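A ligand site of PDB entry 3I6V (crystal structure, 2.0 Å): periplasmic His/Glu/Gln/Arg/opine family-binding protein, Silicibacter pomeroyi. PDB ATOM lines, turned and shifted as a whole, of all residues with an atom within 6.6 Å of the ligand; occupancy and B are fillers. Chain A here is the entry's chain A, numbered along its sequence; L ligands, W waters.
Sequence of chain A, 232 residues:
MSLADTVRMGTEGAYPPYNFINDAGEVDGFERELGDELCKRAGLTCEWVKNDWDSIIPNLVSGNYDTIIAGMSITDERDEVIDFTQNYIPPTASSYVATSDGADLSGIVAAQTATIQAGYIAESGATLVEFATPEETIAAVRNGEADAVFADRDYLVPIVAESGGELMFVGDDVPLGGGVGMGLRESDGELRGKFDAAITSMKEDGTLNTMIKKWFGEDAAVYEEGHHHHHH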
ATOM      1  N   GLU A  12      26.021  22.095  19.400  1.00  0.00           N
ATOM      2  CA  GLU A  12      26.906  22.858  20.269  1.00  0.00           C
ATOM      3  C   GLU A  12      28.324  22.224  20.322  1.00  0.00           C
ATOM      4  O   GLU A  12      29.301  22.952  20.384  1.00  0.00           O
ATOM      5  CB  GLU A  12      26.336  22.902  21.689  1.00  0.00           C
ATOM      6  CG  GLU A  12      27.083  23.812  22.639  1.00  0.00           C
ATOM      7  CD  GLU A  12      26.501  23.819  24.084  1.00  0.00           C
ATOM      8  OE1 GLU A  12      25.607  23.002  24.419  1.00  0.00           O
ATOM      9  OE2 GLU A  12      26.962  24.653  24.888  1.00  0.00           O
ATOM     10  N   ALA A  14      29.590  20.557  22.827  1.00  0.00           N
ATOM     11  CA  ALA A  14      30.141  20.762  24.165  1.00  0.00           C
ATOM     12  C   ALA A  14      29.192  20.301  25.255  1.00  0.00           C
ATOM     13  O   ALA A  14      29.199  20.834  26.354  1.00  0.00           O
ATOM     14  CB  ALA A  14      30.560  22.246  24.362  1.00  0.00           C
ATOM     15  N   TYR A  15      28.398  19.281  24.963  1.00  0.00           N
ATOM     16  CA  TYR A  15      27.328  18.942  25.894  1.00  0.00           C
ATOM     17  C   TYR A  15      27.187  17.434  26.002  1.00  0.00           C
ATOM     18  O   TYR A  15      26.160  16.865  25.617  1.00  0.00           O
ATOM     19  CB  TYR A  15      26.007  19.602  25.405  1.00  0.00           C
ATOM     20  CG  TYR A  15      24.850  19.559  26.374  1.00  0.00           C
ATOM     21  CD1 TYR A  15      25.052  19.767  27.765  1.00  0.00           C
ATOM     22  CD2 TYR A  15      23.548  19.328  25.913  1.00  0.00           C
ATOM     23  CE1 TYR A  15      23.955  19.762  28.672  1.00  0.00           C
ATOM     24  CE2 TYR A  15      22.446  19.323  26.807  1.00  0.00           C
ATOM     25  CZ  TYR A  15      22.672  19.523  28.188  1.00  0.00           C
ATOM     26  OH  TYR A  15      21.623  19.510  29.060  1.00  0.00           O
ATOM     27  N   TYR A  18      24.940  14.193  25.106  1.00  0.00           N
ATOM     28  CA  TYR A  18      24.091  14.579  23.969  1.00  0.00           C
ATOM     29  C   TYR A  18      24.923  14.842  22.703  1.00  0.00           C
ATOM     30  O   TYR A  18      24.666  14.247  21.643  1.00  0.00           O
ATOM     31  CB  TYR A  18      23.320  15.886  24.290  1.00  0.00           C
ATOM     32  CG  TYR A  18      22.391  15.774  25.467  1.00  0.00           C
ATOM     33  CD1 TYR A  18      22.839  16.062  26.761  1.00  0.00           C
ATOM     34  CD2 TYR A  18      21.050  15.399  25.283  1.00  0.00           C
ATOM     35  CE1 TYR A  18      21.968  15.979  27.877  1.00  0.00           C
ATOM     36  CE2 TYR A  18      20.155  15.302  26.393  1.00  0.00           C
ATOM     37  CZ  TYR A  18      20.613  15.607  27.676  1.00  0.00           C
ATOM     38  OH  TYR A  18      19.762  15.535  28.753  1.00  0.00           O
ATOM     39  N   ASN A  19      25.872  15.765  22.833  1.00  0.00           N
ATOM     40  CA  ASN A  19      26.760  16.119  21.733  1.00  0.00           C
ATOM     41  C   ASN A  19      28.148  16.580  22.254  1.00  0.00           C
ATOM     42  O   ASN A  19      28.279  17.146  23.349  1.00  0.00           O
ATOM     43  CB  ASN A  19      26.134  17.202  20.839  1.00  0.00           C
ATOM     44  CG  ASN A  19      25.868  18.503  21.579  1.00  0.00           C
ATOM     45  OD1 ASN A  19      26.786  19.343  21.726  1.00  0.00           O
ATOM     46  ND2 ASN A  19      24.632  18.697  22.033  1.00  0.00           N
ATOM     47  N   TRP A  53      26.504  27.717  21.938  1.00  0.00           N
ATOM     48  CA  TRP A  53      25.136  27.747  22.454  1.00  0.00           C
ATOM     49  C   TRP A  53      24.523  29.144  22.446  1.00  0.00           C
ATOM     50  O   TRP A  53      23.396  29.308  21.980  1.00  0.00           O
ATOM     51  CB  TRP A  53      25.080  27.133  23.855  1.00  0.00           C
ATOM     52  CG  TRP A  53      23.684  27.124  24.411  1.00  0.00           C
ATOM     53  CD1 TRP A  53      23.138  28.051  25.255  1.00  0.00           C
ATOM     54  CD2 TRP A  53      22.633  26.208  24.078  1.00  0.00           C
ATOM     55  NE1 TRP A  53      21.825  27.736  25.514  1.00  0.00           N
ATOM     56  CE2 TRP A  53      21.493  26.604  24.810  1.00  0.00           C
ATOM     57  CE3 TRP A  53      22.562  25.043  23.271  1.00  0.00           C
ATOM     58  CZ2 TRP A  53      20.280  25.902  24.762  1.00  0.00           C
ATOM     59  CZ3 TRP A  53      21.360  24.337  23.218  1.00  0.00           C
ATOM     60  CH2 TRP A  53      20.236  24.761  23.961  1.00  0.00           C
ATOM     61  N   ALA A  70      20.758  19.727  19.664  1.00  0.00           N
ATOM     62  CA  ALA A  70      21.742  20.212  20.639  1.00  0.00           C
ATOM     63  C   ALA A  70      21.133  20.214  22.042  1.00  0.00           C
ATOM     64  O   ALA A  70      21.286  21.188  22.789  1.00  0.00           O
ATOM     65  CB  ALA A  70      22.213  21.662  20.253  1.00  0.00           C
ATOM     66  N   GLY A  71      20.441  19.130  22.378  1.00  0.00           N
ATOM     67  CA  GLY A  71      19.789  18.992  23.707  1.00  0.00           C
ATOM     68  C   GLY A  71      18.857  20.134  24.079  1.00  0.00           C
ATOM     69  O   GLY A  71      18.722  20.457  25.255  1.00  0.00           O
ATOM     70  N   MET A  72      18.205  20.741  23.078  1.00  0.00           N
ATOM     71  CA  MET A  72      17.397  21.977  23.281  1.00  0.00           C
ATOM     72  C   MET A  72      15.958  21.563  23.634  1.00  0.00           C
ATOM     73  O   MET A  72      15.315  20.905  22.823  1.00  0.00           O
ATOM     74  CB  MET A  72      17.367  22.831  22.005  1.00  0.00           C
ATOM     75  CG  MET A  72      16.611  24.223  22.140  1.00  0.00           C
ATOM     76  SD  MET A  72      16.721  25.290  20.688  1.00  0.00           S
ATOM     77  CE  MET A  72      18.292  26.036  21.033  1.00  0.00           C
ATOM     78  N   SER A  73      15.486  21.966  24.809  1.00  0.00           N
ATOM     79  CA  SER A  73      14.107  21.736  25.201  1.00  0.00           C
ATOM     80  C   SER A  73      13.139  22.535  24.357  1.00  0.00           C
ATOM     81  O   SER A  73      13.390  23.714  24.033  1.00  0.00           O
ATOM     82  CB  SER A  73      13.902  22.127  26.663  1.00  0.00           C
ATOM     83  OG  SER A  73      14.610  21.225  27.517  1.00  0.00           O
ATOM     84  N   ILE A  74      12.021  21.895  24.029  1.00  0.00           N
ATOM     85  CA  ILE A  74      10.937  22.563  23.311  1.00  0.00           C
ATOM     86  C   ILE A  74      10.267  23.524  24.307  1.00  0.00           C
ATOM     87  O   ILE A  74       9.845  23.075  25.363  1.00  0.00           O
ATOM     88  CB  ILE A  74       9.923  21.548  22.827  1.00  0.00           C
ATOM     89  CG1 ILE A  74      10.520  20.688  21.728  1.00  0.00           C
ATOM     90  CG2 ILE A  74       8.649  22.258  22.236  1.00  0.00           C
ATOM     91  CD1 ILE A  74       9.802  19.305  21.561  1.00  0.00           C
ATOM     92  N   THR A  75      10.209  24.829  24.026  1.00  0.00           N
ATOM     93  CA  THR A  75       9.501  25.760  24.906  1.00  0.00           C
ATOM     94  C   THR A  75       8.697  26.772  24.090  1.00  0.00           C
ATOM     95  O   THR A  75       9.002  27.027  22.912  1.00  0.00           O
ATOM     96  CB  THR A  75      10.438  26.583  25.803  1.00  0.00           C
ATOM     97  OG1 THR A  75      11.129  27.543  24.992  1.00  0.00           O
ATOM     98  CG2 THR A  75      11.440  25.680  26.550  1.00  0.00           C
ATOM     99  N   ARG A  78      10.787  29.774  22.901  1.00  0.00           N
ATOM    100  CA  ARG A  78      11.644  29.572  21.729  1.00  0.00           C
ATOM    101  C   ARG A  78      10.777  29.407  20.493  1.00  0.00           C
ATOM    102  O   ARG A  78      11.169  29.746  19.406  1.00  0.00           O
ATOM    103  CB  ARG A  78      12.597  28.370  21.867  1.00  0.00           C
ATOM    104  CG  ARG A  78      13.742  28.656  22.856  1.00  0.00           C
ATOM    105  CD  ARG A  78      14.363  27.350  23.348  1.00  0.00           C
ATOM    106  NE  ARG A  78      15.475  27.609  24.265  1.00  0.00           N
ATOM    107  CZ  ARG A  78      15.946  26.733  25.134  1.00  0.00           C
ATOM    108  NH1 ARG A  78      15.344  25.560  25.283  1.00  0.00           N
ATOM    109  NH2 ARG A  78      16.965  27.065  25.925  1.00  0.00           N
ATOM    110  N   SER A  94      15.609  18.559  35.829  1.00  0.00           N
ATOM    111  CA  SER A  94      16.760  19.387  36.131  1.00  0.00           C
ATOM    112  C   SER A  94      17.084  19.193  37.619  1.00  0.00           C
ATOM    113  O   SER A  94      16.186  18.859  38.418  1.00  0.00           O
ATOM    114  CB  SER A  94      16.441  20.842  35.851  1.00  0.00           C
ATOM    115  OG  SER A  94      16.270  21.035  34.453  1.00  0.00           O
ATOM    116  N   GLN A 112      23.972  27.587  32.710  1.00  0.00           N
ATOM    117  CA  GLN A 112      24.319  28.003  31.362  1.00  0.00           C
ATOM    118  C   GLN A 112      23.393  29.100  30.831  1.00  0.00           C
ATOM    119  O   GLN A 112      22.159  29.037  31.003  1.00  0.00           O
ATOM    120  CB  GLN A 112      24.349  26.804  30.404  1.00  0.00           C
ATOM    121  CG  GLN A 112      24.756  27.192  28.952  1.00  0.00           C
ATOM    122  CD  GLN A 112      25.014  25.997  28.068  1.00  0.00           C
ATOM    123  OE1 GLN A 112      24.488  24.922  28.290  1.00  0.00           O
ATOM    124  NE2 GLN A 112      25.845  26.176  27.058  1.00  0.00           N
ATOM    125  N   ALA A 114      21.089  31.361  28.413  1.00  0.00           N
ATOM    126  CA  ALA A 114      20.044  31.021  27.419  1.00  0.00           C
ATOM    127  C   ALA A 114      19.479  29.605  27.577  1.00  0.00           C
ATOM    128  O   ALA A 114      19.252  28.919  26.569  1.00  0.00           O
ATOM    129  CB  ALA A 114      20.575  31.238  25.930  1.00  0.00           C
ATOM    130  N   THR A 115      19.260  29.158  28.817  1.00  0.00           N
ATOM    131  CA  THR A 115      18.653  27.845  29.037  1.00  0.00           C
ATOM    132  C   THR A 115      17.416  27.970  29.941  1.00  0.00           C
ATOM    133  O   THR A 115      17.214  28.982  30.623  1.00  0.00           O
ATOM    134  CB  THR A 115      19.623  26.843  29.738  1.00  0.00           C
ATOM    135  OG1 THR A 115      20.024  27.375  30.995  1.00  0.00           O
ATOM    136  CG2 THR A 115      20.864  26.516  28.845  1.00  0.00           C
ATOM    137  N   ILE A 116      16.607  26.909  29.967  1.00  0.00           N
ATOM    138  CA  ILE A 116      15.427  26.918  30.840  1.00  0.00           C
ATOM    139  C   ILE A 116      15.897  26.926  32.286  1.00  0.00           C
ATOM    140  O   ILE A 116      15.226  27.475  33.161  1.00  0.00           O
ATOM    141  CB  ILE A 116      14.491  25.744  30.538  1.00  0.00           C
ATOM    142  CG1 ILE A 116      15.188  24.401  30.751  1.00  0.00           C
ATOM    143  CG2 ILE A 116      13.996  25.859  29.078  1.00  0.00           C
ATOM    144  CD1 ILE A 116      14.413  23.181  30.279  1.00  0.00           C
ATOM    145  N   GLN A 117      17.088  26.341  32.527  1.00  0.00           N
ATOM    146  CA  GLN A 117      17.647  26.281  33.901  1.00  0.00           C
ATOM    147  C   GLN A 117      18.023  27.665  34.364  1.00  0.00           C
ATOM    148  O   GLN A 117      17.677  28.074  35.487  1.00  0.00           O
ATOM    149  CB  GLN A 117      18.815  25.290  34.000  1.00  0.00           C
ATOM    150  CG  GLN A 117      18.353  23.813  33.959  1.00  0.00           C
ATOM    151  CD  GLN A 117      18.156  23.304  32.534  1.00  0.00           C
ATOM    152  OE1 GLN A 117      18.497  24.010  31.580  1.00  0.00           O
ATOM    153  NE2 GLN A 117      17.596  22.092  32.380  1.00  0.00           N
ATOM    154  N   ALA A 118      18.701  28.425  33.502  1.00  0.00           N
ATOM    155  CA  ALA A 118      18.953  29.837  33.825  1.00  0.00           C
ATOM    156  C   ALA A 118      17.644  30.607  34.057  1.00  0.00           C
ATOM    157  O   ALA A 118      17.567  31.387  34.998  1.00  0.00           O
ATOM    158  CB  ALA A 118      19.763  30.522  32.714  1.00  0.00           C
ATOM    159  N   THR A 133      29.283  28.031  28.590  1.00  0.00           N
ATOM    160  CA  THR A 133      29.355  26.604  28.238  1.00  0.00           C
ATOM    161  C   THR A 133      28.981  25.761  29.437  1.00  0.00           C
ATOM    162  O   THR A 133      29.058  26.243  30.573  1.00  0.00           O
ATOM    163  CB  THR A 133      30.791  26.187  27.796  1.00  0.00           C
ATOM    164  OG1 THR A 133      31.651  26.210  28.950  1.00  0.00           O
ATOM    165  CG2 THR A 133      31.353  27.099  26.653  1.00  0.00           C
ATOM    166  N   PRO A 134      28.597  24.486  29.221  1.00  0.00           N
ATOM    167  CA  PRO A 134      28.238  23.643  30.360  1.00  0.00           C
ATOM    168  C   PRO A 134      29.454  23.382  31.282  1.00  0.00           C
ATOM    169  O   PRO A 134      29.348  23.437  32.525  1.00  0.00           O
ATOM    170  CB  PRO A 134      27.801  22.347  29.683  1.00  0.00           C
ATOM    171  CG  PRO A 134      27.300  22.797  28.282  1.00  0.00           C
ATOM    172  CD  PRO A 134      28.399  23.788  27.932  1.00  0.00           C
ATOM    173  N   ASP A 152      20.618  20.195  33.523  1.00  0.00           N
ATOM    174  CA  ASP A 152      19.909  19.002  33.125  1.00  0.00           C
ATOM    175  C   ASP A 152      20.486  17.806  33.871  1.00  0.00           C
ATOM    176  O   ASP A 152      21.733  17.655  33.966  1.00  0.00           O
ATOM    177  CB  ASP A 152      20.107  18.822  31.638  1.00  0.00           C
ATOM    178  CG  ASP A 152      19.416  17.623  31.117  1.00  0.00           C
ATOM    179  OD1 ASP A 152      18.197  17.709  30.861  1.00  0.00           O
ATOM    180  OD2 ASP A 152      20.140  16.615  30.900  1.00  0.00           O
ATOM    181  N   TYR A 155      22.802  15.445  31.986  1.00  0.00           N
ATOM    182  CA  TYR A 155      24.128  16.006  31.811  1.00  0.00           C
ATOM    183  C   TYR A 155      24.928  15.777  33.115  1.00  0.00           C
ATOM    184  O   TYR A 155      26.118  15.382  33.098  1.00  0.00           O
ATOM    185  CB  TYR A 155      24.038  17.497  31.468  1.00  0.00           C
ATOM    186  CG  TYR A 155      25.380  18.217  31.494  1.00  0.00           C
ATOM    187  CD1 TYR A 155      26.379  17.944  30.543  1.00  0.00           C
ATOM    188  CD2 TYR A 155      25.648  19.173  32.484  1.00  0.00           C
ATOM    189  CE1 TYR A 155      27.623  18.625  30.584  1.00  0.00           C
ATOM    190  CE2 TYR A 155      26.853  19.846  32.533  1.00  0.00           C
ATOM    191  CZ  TYR A 155      27.839  19.558  31.602  1.00  0.00           C
ATOM    192  OH  TYR A 155      29.030  20.243  31.742  1.00  0.00           O
ATOM    193  N   LEU A 176      11.405  20.542  33.954  1.00  0.00           N
ATOM    194  CA  LEU A 176      11.401  21.777  33.164  1.00  0.00           C
ATOM    195  C   LEU A 176      11.386  21.448  31.704  1.00  0.00           C
ATOM    196  O   LEU A 176      12.185  20.598  31.265  1.00  0.00           O
ATOM    197  CB  LEU A 176      12.643  22.649  33.469  1.00  0.00           C
ATOM    198  CG  LEU A 176      12.722  23.459  34.744  1.00  0.00           C
ATOM    199  CD1 LEU A 176      14.103  24.194  34.847  1.00  0.00           C
ATOM    200  CD2 LEU A 176      11.550  24.498  34.819  1.00  0.00           C
ATOM    201  N   VAL A 180      13.472  17.306  24.675  1.00  0.00           N
ATOM    202  CA  VAL A 180      14.399  17.835  23.683  1.00  0.00           C
ATOM    203  C   VAL A 180      13.839  17.584  22.253  1.00  0.00           C
ATOM    204  O   VAL A 180      13.332  16.490  21.953  1.00  0.00           O
ATOM    205  CB  VAL A 180      15.799  17.189  23.895  1.00  0.00           C
ATOM    206  CG1 VAL A 180      16.763  17.694  22.878  1.00  0.00           C
ATOM    207  CG2 VAL A 180      16.343  17.570  25.291  1.00  0.00           C
HETATM  208  N1  LIG L   1      17.467  21.442  27.769  1.00  0.00           N
HETATM  209  C1  LIG L   1      17.879  22.743  28.403  1.00  0.00           C
HETATM  210  C2  LIG L   1      17.427  23.921  27.565  1.00  0.00           C
HETATM  211  O1  LIG L   1      16.935  23.705  26.447  1.00  0.00           O
HETATM  212  C3  LIG L   1      19.416  22.789  28.588  1.00  0.00           C
HETATM  213  C4  LIG L   1      20.232  22.844  27.294  1.00  0.00           C
HETATM  214  C5  LIG L   1      21.762  22.809  27.622  1.00  0.00           C
HETATM  215  C6  LIG L   1      22.672  22.940  26.347  1.00  0.00           C
HETATM  216  N2  LIG L   1      24.161  22.787  26.740  1.00  0.00           N
HETATM  217  O2  LIG L   1      17.552  25.100  27.998  1.00  0.00           O
HETATM  218  O   HOH W   1      19.164  19.083  27.750  1.00  0.00           O
HETATM  219  O   HOH W   2      17.024  20.109  30.533  1.00  0.00           O
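NE2 of Gln 112 is in hydrogen-bond range of OE2 of Glu 12, at 2.9 Å.
O of Gln 112 lies within hydrogen-bond range of OG1 of Thr 115 (2.7 Å).
The guanidinium group (NH1) of Arg 78 lies within hydrogen-bond range of the backbone carbonyl oxygen (O) of Ser 73, 3.0 Å away.
The backbone carbonyl oxygen (O) of Ala 114 sits at hydrogen-bond distance from the guanidinium group (NH2) of Arg 78, at 3.0 Å.
N of Arg 78 is in hydrogen-bond range of OG1 of Thr 75 (3.1 Å).
The side-chain hydroxyl (OG1) of Thr 115 lies close to the backbone NH (N) of Gln 117, 3.5 Å away.
The side-chain hydroxyl (OG1) of Thr 115 sits at hydrogen-bond distance from the backbone NH (N) of Ala 118, 3.0 Å away.
O of Pro 134 lies close to OH of Tyr 155 (3.3 Å).
Water W1 lies within hydrogen-bond range of OH of Tyr 15 (2.8 Å), O of Gly 71 (2.9 Å) and N1 of the ligand (2.9 Å).
Water W2 lies within hydrogen-bond range of OD1 of Asp 152 (2.7 Å), NE2 of Gln 117 (2.8 Å) and N1 of the ligand (3.1 Å).
Residues that only touch the ligand: Thr 115 (3.1 Å), Tyr 15 (3.3 Å), Gln 117 (3.4 Å), Pro 134 (3.5 Å), Met 72 (3.6 Å) and Trp 53 (3.7 Å).
Hydrophobic or aromatic side chains within 4 Å of the ligand: Tyr 15, Trp 53, Ile 116 and Pro 134.
12 residues have an atom within 4 Å of the ligand: Glu 12, Tyr 15, Trp 53, Gly 71, Met 72, Ser 73, Arg 78, Gln 112, Thr 115, Ile 116, Gln 117 and Pro 134.
The nearest printed residue that does not touch the ligand is Ala 70 (4.2 Å).
OE1 of Gln 112 lies within hydrogen-bond range of N2 of the ligand, at 2.7 Å.
The guanidinium group of Arg 78 is in salt-bridge range of an oxygen (O1) of the ligand.
The side-chain carboxylate of Glu 12 lies within salt-bridge range of a nitrogen (N2) of the ligand (2.7 Å).
The backbone NH (N) of Ser 73 lies within hydrogen-bond range of an oxygen (O1) of the ligand (2.8 Å).
OG of Ser 73 lies within hydrogen-bond range of N1 of the ligand (2.9 Å).
N of Ile 116 sits at hydrogen-bond distance from O2 of the ligand.
The backbone carbonyl oxygen (O) of Gly 71 is in hydrogen-bond range of a nitrogen (N1) of the ligand (3.0 Å).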
